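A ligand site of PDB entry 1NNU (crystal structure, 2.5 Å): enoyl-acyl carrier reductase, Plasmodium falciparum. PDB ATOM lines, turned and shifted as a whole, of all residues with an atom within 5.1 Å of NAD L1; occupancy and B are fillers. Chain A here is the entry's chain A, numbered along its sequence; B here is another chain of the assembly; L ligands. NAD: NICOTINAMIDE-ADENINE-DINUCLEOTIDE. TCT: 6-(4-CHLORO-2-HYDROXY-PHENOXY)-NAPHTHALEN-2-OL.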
ATOM      1  N   GLY A   8      29.100 -28.749  20.328  1.00  0.00           N
ATOM      2  CA  GLY A   8      28.709 -27.489  20.918  1.00  0.00           C
ATOM      3  C   GLY A   8      27.291 -27.488  21.433  1.00  0.00           C
ATOM      4  O   GLY A   8      26.449 -26.723  20.959  1.00  0.00           O
ATOM      5  N   ILE A   9      27.011 -28.364  22.386  1.00  0.00           N
ATOM      6  CA  ILE A   9      25.689 -28.459  22.988  1.00  0.00           C
ATOM      7  C   ILE A   9      25.864 -28.584  24.488  1.00  0.00           C
ATOM      8  O   ILE A   9      26.661 -29.398  24.953  1.00  0.00           O
ATOM      9  CB  ILE A   9      24.898 -29.666  22.481  1.00  0.00           C
ATOM     10  CG1 ILE A   9      24.516 -29.460  21.016  1.00  0.00           C
ATOM     11  CG2 ILE A   9      23.642 -29.858  23.294  1.00  0.00           C
ATOM     12  CD1 ILE A   9      23.623 -30.548  20.449  1.00  0.00           C
ATOM     13  N   GLY A  10      25.138 -27.770  25.240  1.00  0.00           N
ATOM     14  CA  GLY A  10      25.221 -27.819  26.688  1.00  0.00           C
ATOM     15  C   GLY A  10      23.833 -27.749  27.274  1.00  0.00           C
ATOM     16  O   GLY A  10      23.651 -27.837  28.483  1.00  0.00           O
ATOM     17  N   ASP A  11      22.842 -27.583  26.413  1.00  0.00           N
ATOM     18  CA  ASP A  11      21.463 -27.467  26.848  1.00  0.00           C
ATOM     19  C   ASP A  11      20.519 -27.468  25.661  1.00  0.00           C
ATOM     20  O   ASP A  11      20.919 -27.777  24.536  1.00  0.00           O
ATOM     21  CB  ASP A  11      21.288 -26.173  27.646  1.00  0.00           C
ATOM     22  CG  ASP A  11      21.827 -24.971  26.903  1.00  0.00           C
ATOM     23  OD1 ASP A  11      21.348 -24.699  25.779  1.00  0.00           O
ATOM     24  OD2 ASP A  11      22.745 -24.314  27.436  1.00  0.00           O
ATOM     25  N   ASN A  13      18.615 -24.661  24.945  1.00  0.00           N
ATOM     26  CA  ASN A  13      18.310 -23.263  24.640  1.00  0.00           C
ATOM     27  C   ASN A  13      19.196 -22.644  23.557  1.00  0.00           C
ATOM     28  O   ASN A  13      19.073 -21.460  23.266  1.00  0.00           O
ATOM     29  CB  ASN A  13      18.435 -22.423  25.908  1.00  0.00           C
ATOM     30  CG  ASN A  13      17.711 -23.033  27.080  1.00  0.00           C
ATOM     31  OD1 ASN A  13      16.551 -23.439  26.978  1.00  0.00           O
ATOM     32  ND2 ASN A  13      18.381 -23.100  28.216  1.00  0.00           N
ATOM     33  N   GLY A  14      20.071 -23.430  22.966  1.00  0.00           N
ATOM     34  CA  GLY A  14      20.940 -22.897  21.941  1.00  0.00           C
ATOM     35  C   GLY A  14      20.519 -23.292  20.550  1.00  0.00           C
ATOM     36  O   GLY A  14      19.468 -23.899  20.370  1.00  0.00           O
ATOM     37  N   TYR A  15      21.355 -22.947  19.579  1.00  0.00           N
ATOM     38  CA  TYR A  15      21.102 -23.273  18.178  1.00  0.00           C
ATOM     39  C   TYR A  15      21.408 -24.745  17.859  1.00  0.00           C
ATOM     40  O   TYR A  15      20.774 -25.332  16.984  1.00  0.00           O
ATOM     41  CB  TYR A  15      21.957 -22.384  17.266  1.00  0.00           C
ATOM     42  CG  TYR A  15      21.346 -21.039  16.955  1.00  0.00           C
ATOM     43  CD1 TYR A  15      20.087 -20.947  16.370  1.00  0.00           C
ATOM     44  CD2 TYR A  15      22.039 -19.852  17.214  1.00  0.00           C
ATOM     45  CE1 TYR A  15      19.535 -19.711  16.032  1.00  0.00           C
ATOM     46  CE2 TYR A  15      21.496 -18.608  16.882  1.00  0.00           C
ATOM     47  CZ  TYR A  15      20.246 -18.548  16.293  1.00  0.00           C
ATOM     48  OH  TYR A  15      19.699 -17.333  15.959  1.00  0.00           O
ATOM     49  N   GLY A  16      22.386 -25.307  18.559  1.00  0.00           N
ATOM     50  CA  GLY A  16      22.757 -26.694  18.332  1.00  0.00           C
ATOM     51  C   GLY A  16      21.549 -27.576  18.517  1.00  0.00           C
ATOM     52  O   GLY A  16      21.324 -28.521  17.749  1.00  0.00           O
ATOM     53  N   TRP A  35      30.777 -30.286  25.903  1.00  0.00           N
ATOM     54  CA  TRP A  35      31.934 -29.708  26.584  1.00  0.00           C
ATOM     55  C   TRP A  35      32.008 -30.344  27.980  1.00  0.00           C
ATOM     56  O   TRP A  35      31.061 -30.268  28.754  1.00  0.00           O
ATOM     57  CB  TRP A  35      31.738 -28.193  26.668  1.00  0.00           C
ATOM     58  CG  TRP A  35      32.911 -27.425  27.161  1.00  0.00           C
ATOM     59  CD1 TRP A  35      34.226 -27.681  26.890  1.00  0.00           C
ATOM     60  CD2 TRP A  35      32.873 -26.252  27.970  1.00  0.00           C
ATOM     61  NE1 TRP A  35      35.017 -26.723  27.481  1.00  0.00           N
ATOM     62  CE2 TRP A  35      34.214 -25.836  28.147  1.00  0.00           C
ATOM     63  CE3 TRP A  35      31.846 -25.499  28.549  1.00  0.00           C
ATOM     64  CZ2 TRP A  35      34.558 -24.696  28.893  1.00  0.00           C
ATOM     65  CZ3 TRP A  35      32.183 -24.364  29.298  1.00  0.00           C
ATOM     66  CH2 TRP A  35      33.531 -23.983  29.461  1.00  0.00           C
ATOM     67  N   VAL A  38      30.321 -29.281  31.488  1.00  0.00           N
ATOM     68  CA  VAL A  38      28.871 -29.372  31.653  1.00  0.00           C
ATOM     69  C   VAL A  38      28.313 -30.711  31.182  1.00  0.00           C
ATOM     70  O   VAL A  38      27.102 -30.867  31.028  1.00  0.00           O
ATOM     71  CB  VAL A  38      28.138 -28.237  30.873  1.00  0.00           C
ATOM     72  CG1 VAL A  38      28.835 -26.908  31.117  1.00  0.00           C
ATOM     73  CG2 VAL A  38      28.081 -28.555  29.386  1.00  0.00           C
ATOM     74  N   PHE A  71      33.418 -33.712  24.825  1.00  0.00           N
ATOM     75  CA  PHE A  71      34.219 -33.189  23.712  1.00  0.00           C
ATOM     76  C   PHE A  71      34.686 -31.760  23.969  1.00  0.00           C
ATOM     77  O   PHE A  71      33.889 -30.885  24.269  1.00  0.00           O
ATOM     78  CB  PHE A  71      33.354 -33.237  22.435  1.00  0.00           C
ATOM     79  CG  PHE A  71      33.939 -32.493  21.270  1.00  0.00           C
ATOM     80  CD1 PHE A  71      34.861 -33.106  20.436  1.00  0.00           C
ATOM     81  CD2 PHE A  71      33.530 -31.189  20.989  1.00  0.00           C
ATOM     82  CE1 PHE A  71      35.374 -32.429  19.325  1.00  0.00           C
ATOM     83  CE2 PHE A  71      34.037 -30.504  19.877  1.00  0.00           C
ATOM     84  CZ  PHE A  71      34.958 -31.130  19.047  1.00  0.00           C
ATOM     85  N   ASP A  72      35.985 -31.545  23.826  1.00  0.00           N
ATOM     86  CA  ASP A  72      36.567 -30.219  24.043  1.00  0.00           C
ATOM     87  C   ASP A  72      37.334 -29.773  22.798  1.00  0.00           C
ATOM     88  O   ASP A  72      38.388 -30.305  22.473  1.00  0.00           O
ATOM     89  CB  ASP A  72      37.503 -30.249  25.250  1.00  0.00           C
ATOM     90  CG  ASP A  72      37.838 -28.880  25.752  1.00  0.00           C
ATOM     91  OD1 ASP A  72      38.153 -28.005  24.917  1.00  0.00           O
ATOM     92  OD2 ASP A  72      37.798 -28.660  26.979  1.00  0.00           O
ATOM     93  N   ALA A  73      36.783 -28.782  22.099  1.00  0.00           N
ATOM     94  CA  ALA A  73      37.377 -28.281  20.857  1.00  0.00           C
ATOM     95  C   ALA A  73      38.744 -27.618  20.976  1.00  0.00           C
ATOM     96  O   ALA A  73      39.378 -27.323  19.966  1.00  0.00           O
ATOM     97  CB  ALA A  73      36.402 -27.331  20.175  1.00  0.00           C
ATOM     98  N   SER A  74      39.205 -27.398  22.202  1.00  0.00           N
ATOM     99  CA  SER A  74      40.506 -26.759  22.373  1.00  0.00           C
ATOM    100  C   SER A  74      41.664 -27.742  22.403  1.00  0.00           C
ATOM    101  O   SER A  74      42.817 -27.318  22.491  1.00  0.00           O
ATOM    102  CB  SER A  74      40.514 -25.909  23.633  1.00  0.00           C
ATOM    103  OG  SER A  74      40.427 -26.706  24.788  1.00  0.00           O
ATOM    104  N   SER A 119      28.951 -25.760  16.263  1.00  0.00           N
ATOM    105  CA  SER A 119      28.057 -24.784  16.874  1.00  0.00           C
ATOM    106  C   SER A 119      28.549 -24.397  18.261  1.00  0.00           C
ATOM    107  O   SER A 119      27.812 -24.470  19.238  1.00  0.00           O
ATOM    108  CB  SER A 119      26.652 -25.393  16.991  1.00  0.00           C
ATOM    109  OG  SER A 119      25.793 -24.568  17.759  1.00  0.00           O
ATOM    110  N   LEU A 120      29.803 -23.957  18.335  1.00  0.00           N
ATOM    111  CA  LEU A 120      30.390 -23.581  19.610  1.00  0.00           C
ATOM    112  C   LEU A 120      31.240 -22.326  19.471  1.00  0.00           C
ATOM    113  O   LEU A 120      31.754 -22.017  18.388  1.00  0.00           O
ATOM    114  CB  LEU A 120      31.256 -24.732  20.134  1.00  0.00           C
ATOM    115  CG  LEU A 120      32.523 -25.068  19.335  1.00  0.00           C
ATOM    116  CD1 LEU A 120      33.755 -24.677  20.141  1.00  0.00           C
ATOM    117  CD2 LEU A 120      32.571 -26.539  19.030  1.00  0.00           C
ATOM    118  N   ALA A 121      31.395 -21.603  20.563  1.00  0.00           N
ATOM    119  CA  ALA A 121      32.203 -20.395  20.592  1.00  0.00           C
ATOM    120  C   ALA A 121      32.681 -20.208  22.022  1.00  0.00           C
ATOM    121  O   ALA A 121      32.093 -20.742  22.956  1.00  0.00           O
ATOM    122  CB  ALA A 121      31.378 -19.194  20.131  1.00  0.00           C
ATOM    123  N   ASN A 122      33.765 -19.460  22.192  1.00  0.00           N
ATOM    124  CA  ASN A 122      34.278 -19.215  23.526  1.00  0.00           C
ATOM    125  C   ASN A 122      35.264 -18.073  23.513  1.00  0.00           C
ATOM    126  O   ASN A 122      36.224 -18.074  22.749  1.00  0.00           O
ATOM    127  CB  ASN A 122      34.943 -20.485  24.080  1.00  0.00           C
ATOM    128  CG  ASN A 122      35.131 -20.433  25.586  1.00  0.00           C
ATOM    129  OD1 ASN A 122      36.055 -19.799  26.092  1.00  0.00           O
ATOM    130  ND2 ASN A 122      34.238 -21.099  26.302  1.00  0.00           N
ATOM    131  N   LYS A 144      39.596 -21.450  20.312  1.00  0.00           N
ATOM    132  CA  LYS A 144      38.363 -22.175  20.632  1.00  0.00           C
ATOM    133  C   LYS A 144      37.223 -21.958  19.632  1.00  0.00           C
ATOM    134  O   LYS A 144      36.479 -22.882  19.318  1.00  0.00           O
ATOM    135  CB  LYS A 144      37.842 -21.775  22.023  1.00  0.00           C
ATOM    136  CG  LYS A 144      38.339 -22.578  23.202  1.00  0.00           C
ATOM    137  CD  LYS A 144      39.712 -22.141  23.661  1.00  0.00           C
ATOM    138  CE  LYS A 144      39.956 -22.535  25.119  1.00  0.00           C
ATOM    139  NZ  LYS A 144      39.045 -21.791  26.033  1.00  0.00           N
ATOM    140  N   LEU A 169      28.282 -21.758  12.761  1.00  0.00           N
ATOM    141  CA  LEU A 169      27.459 -20.576  12.989  1.00  0.00           C
ATOM    142  C   LEU A 169      28.337 -19.341  13.144  1.00  0.00           C
ATOM    143  O   LEU A 169      29.392 -19.386  13.771  1.00  0.00           O
ATOM    144  CB  LEU A 169      26.586 -20.762  14.234  1.00  0.00           C
ATOM    145  CG  LEU A 169      25.409 -21.740  14.184  1.00  0.00           C
ATOM    146  CD1 LEU A 169      24.466 -21.337  13.075  1.00  0.00           C
ATOM    147  CD2 LEU A 169      25.914 -23.137  13.941  1.00  0.00           C
ATOM    148  N   THR A 170      27.907 -18.229  12.579  1.00  0.00           N
ATOM    149  CA  THR A 170      28.683 -17.013  12.708  1.00  0.00           C
ATOM    150  C   THR A 170      27.738 -15.860  13.001  1.00  0.00           C
ATOM    151  O   THR A 170      26.528 -16.047  13.087  1.00  0.00           O
ATOM    152  CB  THR A 170      29.526 -16.727  11.413  1.00  0.00           C
ATOM    153  OG1 THR A 170      30.351 -15.568  11.620  1.00  0.00           O
ATOM    154  CG2 THR A 170      28.632 -16.511  10.203  1.00  0.00           C
ATOM    155  N   TYR A 171      28.294 -14.673  13.185  1.00  0.00           N
ATOM    156  CA  TYR A 171      27.484 -13.513  13.500  1.00  0.00           C
ATOM    157  C   TYR A 171      27.989 -12.344  12.677  1.00  0.00           C
ATOM    158  O   TYR A 171      29.193 -12.182  12.494  1.00  0.00           O
ATOM    159  CB  TYR A 171      27.577 -13.216  15.006  1.00  0.00           C
ATOM    160  CG  TYR A 171      26.714 -12.072  15.484  1.00  0.00           C
ATOM    161  CD1 TYR A 171      25.363 -12.021  15.150  1.00  0.00           C
ATOM    162  CD2 TYR A 171      27.242 -11.041  16.249  1.00  0.00           C
ATOM    163  CE1 TYR A 171      24.562 -10.961  15.562  1.00  0.00           C
ATOM    164  CE2 TYR A 171      26.450  -9.972  16.667  1.00  0.00           C
ATOM    165  CZ  TYR A 171      25.108  -9.941  16.316  1.00  0.00           C
ATOM    166  OH  TYR A 171      24.324  -8.871  16.690  1.00  0.00           O
ATOM    167  N   TYR A 181      30.087  -6.934  21.539  1.00  0.00           N
ATOM    168  CA  TYR A 181      30.574  -8.223  21.062  1.00  0.00           C
ATOM    169  C   TYR A 181      32.094  -8.142  21.053  1.00  0.00           C
ATOM    170  O   TYR A 181      32.723  -8.161  19.995  1.00  0.00           O
ATOM    171  CB  TYR A 181      30.070  -8.443  19.635  1.00  0.00           C
ATOM    172  CG  TYR A 181      30.078  -9.883  19.162  1.00  0.00           C
ATOM    173  CD1 TYR A 181      29.225 -10.836  19.732  1.00  0.00           C
ATOM    174  CD2 TYR A 181      30.924 -10.291  18.135  1.00  0.00           C
ATOM    175  CE1 TYR A 181      29.211 -12.152  19.274  1.00  0.00           C
ATOM    176  CE2 TYR A 181      30.915 -11.603  17.666  1.00  0.00           C
ATOM    177  CZ  TYR A 181      30.054 -12.524  18.239  1.00  0.00           C
ATOM    178  OH  TYR A 181      30.010 -13.813  17.761  1.00  0.00           O
ATOM    179  N   MET A 185      35.611 -11.904  19.713  1.00  0.00           N
ATOM    180  CA  MET A 185      34.611 -12.761  19.090  1.00  0.00           C
ATOM    181  C   MET A 185      34.473 -12.308  17.647  1.00  0.00           C
ATOM    182  O   MET A 185      34.508 -13.121  16.727  1.00  0.00           O
ATOM    183  CB  MET A 185      33.252 -12.634  19.792  1.00  0.00           C
ATOM    184  CG  MET A 185      33.052 -13.652  20.901  1.00  0.00           C
ATOM    185  SD  MET A 185      33.400 -15.340  20.343  1.00  0.00           S
ATOM    186  CE  MET A 185      32.173 -15.507  19.090  1.00  0.00           C
ATOM    187  N   LYS A 189      34.940 -14.589  14.412  1.00  0.00           N
ATOM    188  CA  LYS A 189      33.876 -14.833  13.448  1.00  0.00           C
ATOM    189  C   LYS A 189      34.346 -14.443  12.049  1.00  0.00           C
ATOM    190  O   LYS A 189      33.954 -15.064  11.057  1.00  0.00           O
ATOM    191  CB  LYS A 189      32.616 -14.063  13.842  1.00  0.00           C
ATOM    192  CG  LYS A 189      31.943 -14.587  15.107  1.00  0.00           C
ATOM    193  CD  LYS A 189      31.656 -16.093  14.988  1.00  0.00           C
ATOM    194  CE  LYS A 189      30.829 -16.605  16.157  1.00  0.00           C
ATOM    195  NZ  LYS A 189      30.585 -18.073  16.083  1.00  0.00           N
ATOM    196  N   ALA A 216      23.610 -16.326  11.887  1.00  0.00           N
ATOM    197  CA  ALA A 216      22.327 -16.243  12.563  1.00  0.00           C
ATOM    198  C   ALA A 216      22.003 -14.911  13.226  1.00  0.00           C
ATOM    199  O   ALA A 216      22.890 -14.106  13.507  1.00  0.00           O
ATOM    200  CB  ALA A 216      22.213 -17.353  13.582  1.00  0.00           C
ATOM    201  N   GLY A 217      20.710 -14.729  13.478  1.00  0.00           N
ATOM    202  CA  GLY A 217      20.235 -13.543  14.147  1.00  0.00           C
ATOM    203  C   GLY A 217      20.347 -13.796  15.639  1.00  0.00           C
ATOM    204  O   GLY A 217      20.851 -14.836  16.034  1.00  0.00           O
ATOM    205  N   PRO A 218      19.841 -12.889  16.489  1.00  0.00           N
ATOM    206  CA  PRO A 218      19.912 -13.035  17.953  1.00  0.00           C
ATOM    207  C   PRO A 218      19.022 -14.134  18.514  1.00  0.00           C
ATOM    208  O   PRO A 218      17.901 -14.333  18.047  1.00  0.00           O
ATOM    209  CB  PRO A 218      19.473 -11.654  18.460  1.00  0.00           C
ATOM    210  CG  PRO A 218      19.461 -10.762  17.239  1.00  0.00           C
ATOM    211  CD  PRO A 218      19.079 -11.679  16.139  1.00  0.00           C
ATOM    212  N   LEU A 219      19.529 -14.841  19.509  1.00  0.00           N
ATOM    213  CA  LEU A 219      18.785 -15.906  20.168  1.00  0.00           C
ATOM    214  C   LEU A 219      19.168 -15.880  21.648  1.00  0.00           C
ATOM    215  O   LEU A 219      20.348 -15.976  21.998  1.00  0.00           O
ATOM    216  CB  LEU A 219      19.159 -17.270  19.566  1.00  0.00           C
ATOM    217  CG  LEU A 219      18.509 -18.504  20.204  1.00  0.00           C
ATOM    218  CD1 LEU A 219      17.059 -18.631  19.746  1.00  0.00           C
ATOM    219  CD2 LEU A 219      19.284 -19.750  19.802  1.00  0.00           C
ATOM    220  N   SER A 221      20.135 -17.446  24.149  1.00  0.00           N
ATOM    221  CA  SER A 221      20.691 -18.724  24.582  1.00  0.00           C
ATOM    222  C   SER A 221      21.457 -18.497  25.887  1.00  0.00           C
ATOM    223  O   SER A 221      21.623 -17.356  26.324  1.00  0.00           O
ATOM    224  CB  SER A 221      21.636 -19.286  23.509  1.00  0.00           C
ATOM    225  OG  SER A 221      22.761 -18.447  23.299  1.00  0.00           O
ATOM    226  N   ARG A 222      21.929 -19.570  26.497  1.00  0.00           N
ATOM    227  CA  ARG A 222      22.658 -19.428  27.747  1.00  0.00           C
ATOM    228  C   ARG A 222      23.911 -18.572  27.591  1.00  0.00           C
ATOM    229  O   ARG A 222      24.180 -17.703  28.421  1.00  0.00           O
ATOM    230  CB  ARG A 222      23.045 -20.790  28.321  1.00  0.00           C
ATOM    231  CG  ARG A 222      23.632 -20.648  29.708  1.00  0.00           C
ATOM    232  CD  ARG A 222      24.404 -21.879  30.177  1.00  0.00           C
ATOM    233  NE  ARG A 222      24.992 -21.651  31.500  1.00  0.00           N
ATOM    234  CZ  ARG A 222      25.853 -20.675  31.776  1.00  0.00           C
ATOM    235  NH1 ARG A 222      26.254 -19.830  30.836  1.00  0.00           N
ATOM    236  NH2 ARG A 222      26.313 -20.530  33.020  1.00  0.00           N
ATOM    237  N   ALA A 223      24.680 -18.838  26.544  1.00  0.00           N
ATOM    238  CA  ALA A 223      25.905 -18.102  26.287  1.00  0.00           C
ATOM    239  C   ALA A 223      25.620 -16.639  25.960  1.00  0.00           C
ATOM    240  O   ALA A 223      26.419 -15.758  26.295  1.00  0.00           O
ATOM    241  CB  ALA A 223      26.673 -18.746  25.146  1.00  0.00           C
ATOM    242  N   ALA A 224      24.501 -16.391  25.296  1.00  0.00           N
ATOM    243  CA  ALA A 224      24.120 -15.034  24.922  1.00  0.00           C
ATOM    244  C   ALA A 224      23.906 -14.195  26.169  1.00  0.00           C
ATOM    245  O   ALA A 224      24.321 -13.041  26.233  1.00  0.00           O
ATOM    246  CB  ALA A 224      22.843 -15.054  24.085  1.00  0.00           C
ATOM    247  N   ILE B   4      22.049  -9.112  24.799  1.00  0.00           N
ATOM    248  CA  ILE B   4      21.185  -9.954  23.985  1.00  0.00           C
ATOM    249  C   ILE B   4      19.760  -9.454  23.923  1.00  0.00           C
ATOM    250  O   ILE B   4      19.108  -9.569  22.881  1.00  0.00           O
ATOM    251  CB  ILE B   4      21.186 -11.425  24.479  1.00  0.00           C
ATOM    252  CG1 ILE B   4      20.518 -12.322  23.426  1.00  0.00           C
ATOM    253  CG2 ILE B   4      20.423 -11.542  25.799  1.00  0.00           C
ATOM    254  CD1 ILE B   4      21.242 -12.339  22.085  1.00  0.00           C
HETATM  255  PA  NAD L   1      25.229 -22.108  23.244  1.00  0.00           P
HETATM  256  O1A NAD L   1      24.218 -23.204  23.283  1.00  0.00           O
HETATM  257  O2A NAD L   1      25.571 -21.400  24.541  1.00  0.00           O
HETATM  258  O5B NAD L   1      26.551 -22.810  22.610  1.00  0.00           O
HETATM  259  C5B NAD L   1      27.926 -22.683  23.010  1.00  0.00           C
HETATM  260  C4B NAD L   1      28.447 -24.019  23.380  1.00  0.00           C
HETATM  261  O4B NAD L   1      29.880 -24.180  23.123  1.00  0.00           O
HETATM  262  C3B NAD L   1      28.237 -24.324  24.860  1.00  0.00           C
HETATM  263  O3B NAD L   1      27.141 -25.280  24.924  1.00  0.00           O
HETATM  264  C2B NAD L   1      29.565 -24.878  25.366  1.00  0.00           C
HETATM  265  O2B NAD L   1      29.333 -26.024  26.156  1.00  0.00           O
HETATM  266  C1B NAD L   1      30.413 -25.101  24.071  1.00  0.00           C
HETATM  267  N9A NAD L   1      31.848 -24.778  24.241  1.00  0.00           N
HETATM  268  C8A NAD L   1      32.718 -23.785  24.637  1.00  0.00           C
HETATM  269  N7A NAD L   1      34.003 -24.073  24.591  1.00  0.00           N
HETATM  270  C5A NAD L   1      34.015 -25.381  24.116  1.00  0.00           C
HETATM  271  C6A NAD L   1      35.049 -26.270  23.853  1.00  0.00           C
HETATM  272  N6A NAD L   1      36.333 -25.975  24.052  1.00  0.00           N
HETATM  273  N1A NAD L   1      34.743 -27.498  23.395  1.00  0.00           N
HETATM  274  C2A NAD L   1      33.447 -27.806  23.140  1.00  0.00           C
HETATM  275  N3A NAD L   1      32.356 -27.089  23.426  1.00  0.00           N
HETATM  276  C4A NAD L   1      32.697 -25.834  23.891  1.00  0.00           C
HETATM  277  O3  NAD L   1      24.981 -20.846  22.434  1.00  0.00           O
HETATM  278  PN  NAD L   1      24.582 -20.573  21.019  1.00  0.00           P
HETATM  279  O1N NAD L   1      23.498 -21.463  20.516  1.00  0.00           O
HETATM  280  O2N NAD L   1      24.387 -19.104  20.988  1.00  0.00           O
HETATM  281  O5D NAD L   1      25.979 -20.650  20.244  1.00  0.00           O
HETATM  282  C5D NAD L   1      26.297 -21.640  19.265  1.00  0.00           C
HETATM  283  C4D NAD L   1      26.877 -20.944  18.029  1.00  0.00           C
HETATM  284  O4D NAD L   1      25.890 -20.036  17.434  1.00  0.00           O
HETATM  285  C3D NAD L   1      28.117 -20.121  18.399  1.00  0.00           C
HETATM  286  O3D NAD L   1      29.102 -20.424  17.453  1.00  0.00           O
HETATM  287  C2D NAD L   1      27.611 -18.727  18.274  1.00  0.00           C
HETATM  288  O2D NAD L   1      28.659 -17.851  18.009  1.00  0.00           O
HETATM  289  C1D NAD L   1      26.630 -18.844  17.135  1.00  0.00           C
HETATM  290  N1N NAD L   1      25.725 -17.695  16.968  1.00  0.00           N
HETATM  291  C2N NAD L   1      24.806 -17.409  18.009  1.00  0.00           C
HETATM  292  C3N NAD L   1      23.899 -16.358  18.077  1.00  0.00           C
HETATM  293  C7N NAD L   1      22.935 -16.066  19.149  1.00  0.00           C
HETATM  294  O7N NAD L   1      22.239 -14.924  19.222  1.00  0.00           O
HETATM  295  N7N NAD L   1      22.698 -16.850  20.185  1.00  0.00           N
HETATM  296  C4N NAD L   1      23.927 -15.650  16.873  1.00  0.00           C
HETATM  297  C5N NAD L   1      24.747 -15.896  15.726  1.00  0.00           C
HETATM  298  C6N NAD L   1      25.704 -16.972  15.801  1.00  0.00           C
HETATM  299  C16 TCT L   2      29.531 -18.584  23.081  1.00  0.00           C
HETATM  300  C15 TCT L   2      28.548 -18.290  22.123  1.00  0.00           C
HETATM  301  C14 TCT L   2      28.168 -16.950  21.848  1.00  0.00           C
HETATM  302  C13 TCT L   2      28.792 -15.861  22.536  1.00  0.00           C
HETATM  303  C12 TCT L   2      29.788 -16.131  23.506  1.00  0.00           C
HETATM  304  C11 TCT L   2      30.174 -17.543  23.788  1.00  0.00           C
HETATM  305  C10 TCT L   2      31.168 -17.815  24.748  1.00  0.00           C
HETATM  306  C9  TCT L   2      31.793 -16.763  25.435  1.00  0.00           C
HETATM  307  O3  TCT L   2      32.750 -17.054  26.366  1.00  0.00           O
HETATM  308  C8  TCT L   2      31.438 -15.415  25.174  1.00  0.00           C
HETATM  309  C7  TCT L   2      30.444 -15.091  24.211  1.00  0.00           C
HETATM  310  O2  TCT L   2      27.152 -16.772  20.884  1.00  0.00           O
HETATM  311  C3  TCT L   2      26.585 -15.552  20.479  1.00  0.00           C
HETATM  312  C4  TCT L   2      25.542 -14.975  21.275  1.00  0.00           C
HETATM  313  C5  TCT L   2      24.911 -13.766  20.886  1.00  0.00           C
HETATM  314  C6  TCT L   2      25.309 -13.096  19.706  1.00  0.00           C
HETATM  315 CL1  TCT L   2      24.511 -11.604  19.241  1.00  0.00          CL
HETATM  316  C1  TCT L   2      26.363 -13.652  18.914  1.00  0.00           C
HETATM  317  C2  TCT L   2      27.006 -14.876  19.303  1.00  0.00           C
HETATM  318  O1  TCT L   2      28.003 -15.400  18.526  1.00  0.00           O
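O2D of NAD L1 is in hydrogen-bond range of O1 of TCT L2, 2.6 Å away.
NZ of Lys 189 is in hydrogen-bond range of O of Leu 169 (2.9 Å).
OH of Tyr 15 is in hydrogen-bond range of O of Gly 217, at 2.8 Å.
The side-chain carboxylate (OD2) of Asp 72 sits at hydrogen-bond distance from the indole nitrogen (NE1) of Trp 35.
OD1 of Asp 72 is in hydrogen-bond range of OG of Ser 74, 2.6 Å away.
The side-chain hydroxyl of Ser 221 is in hydrogen-bond range of the backbone NH of Ala 224, 3.4 Å away.
The backbone carbonyl oxygen (O) of Thr 170 is in hydrogen-bond range of the backbone NH (N) of Ala 216 (3.2 Å).
The backbone NH (N) of Gly 14 lies within hydrogen-bond range of the side-chain carboxylate (OD1) of Asp 11 (3.3 Å).
The backbone carbonyl oxygen (O) of Gly 217 lies close to an oxygen (O7N) of NAD L1.
Ile 9 touches NAD L1 (C to O3B, 3.6 Å).
Gly 14 touches NAD L1.
CB of Trp 35 touches O2B of NAD L1, 3.3 Å away.
Phe 71 touches NAD L1 (O to C2A, 3.3 Å).
N of Ser 74 touches N6A of NAD L1 (3.7 Å).
Ser 119 touches NAD L1 (O to C5D, 3.2 Å).
O of Ala 121 touches C8A of NAD L1, 3.5 Å away.
CB of Leu 169 touches O4D of NAD L1, at 3.4 Å.
Thr 170 touches NAD L1.
Tyr 171 touches NAD L1.
Ala 216 touches NAD L1.
Pro 218 touches NAD L1 (CA to O7N, 3.3 Å).
Ile 4 of chain B touches NAD L1 (CD1 to O7N, 3.98 Å).
Hydrophobic or aromatic side chains within 4 Å of NAD L1: Tyr 15, Trp 35, Ala 73, Leu 120, Ala 121, Leu 169, Tyr 171, Ala 216, Leu 219, Ala 223 and Ile 4 of chain B.
Within 4 Å of NAD L1: Ile 9, Gly 10, Gly 14, Tyr 15, Trp 35, Phe 71, Asp 72, Ala 73, Ser 74, Ser 119, Leu 120, Ala 121, Asn 122, Leu 169, Thr 170, Tyr 171, Lys 189, Ala 216, Gly 217, Pro 218, Leu 219, Ser 221, Ala 223 and Ile 4 of chain B.
Along chain A the residues within 4 Å of NAD L1 span positions 9 to 223.
The nearest printed residue that does not touch NAD L1 is Lys 144 (4.04 Å).
O7N of NAD L1 lies within hydrogen-bond range of N of Leu 219 (2.7 Å).
The backbone carbonyl oxygen (O) of Leu 219 is in hydrogen-bond range of a nitrogen (N7N) of NAD L1 (3.1 Å).
An oxygen (O2D) of NAD L1 lies within hydrogen-bond range of the side-chain amino group (NZ) of Lys 189 (2.7 Å).
N1A of NAD L1 sits at hydrogen-bond distance from N of Ala 73.
The backbone NH (N) of Tyr 15 lies within hydrogen-bond range of an oxygen (O1N) of NAD L1, at 2.8 Å.
The side-chain carboxylate (OD1) of Asp 72 lies within hydrogen-bond range of a nitrogen (N6A) of NAD L1, at 2.9 Å.
The side-chain hydroxyl of Ser 221 is in hydrogen-bond range of an oxygen (O2N) of NAD L1 (2.9 Å).
An oxygen (O2A) of NAD L1 lies close to the backbone NH (N) of Ala 223 (3.4 Å).
An oxygen (O3B) of NAD L1 is in hydrogen-bond range of the backbone NH (N) of Gly 10, at 3.2 Å.
The backbone carbonyl oxygen (O) of Leu 120 is in hydrogen-bond range of an oxygen (O3D) of NAD L1 (3.2 Å).
A nitrogen (N7A) of NAD L1 sits at hydrogen-bond distance from the side-chain amide nitrogen of Asn 122 (3.4 Å).
O1 of TCT L2 lies within hydrogen-bond range of OH of Tyr 181 (2.7 Å).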
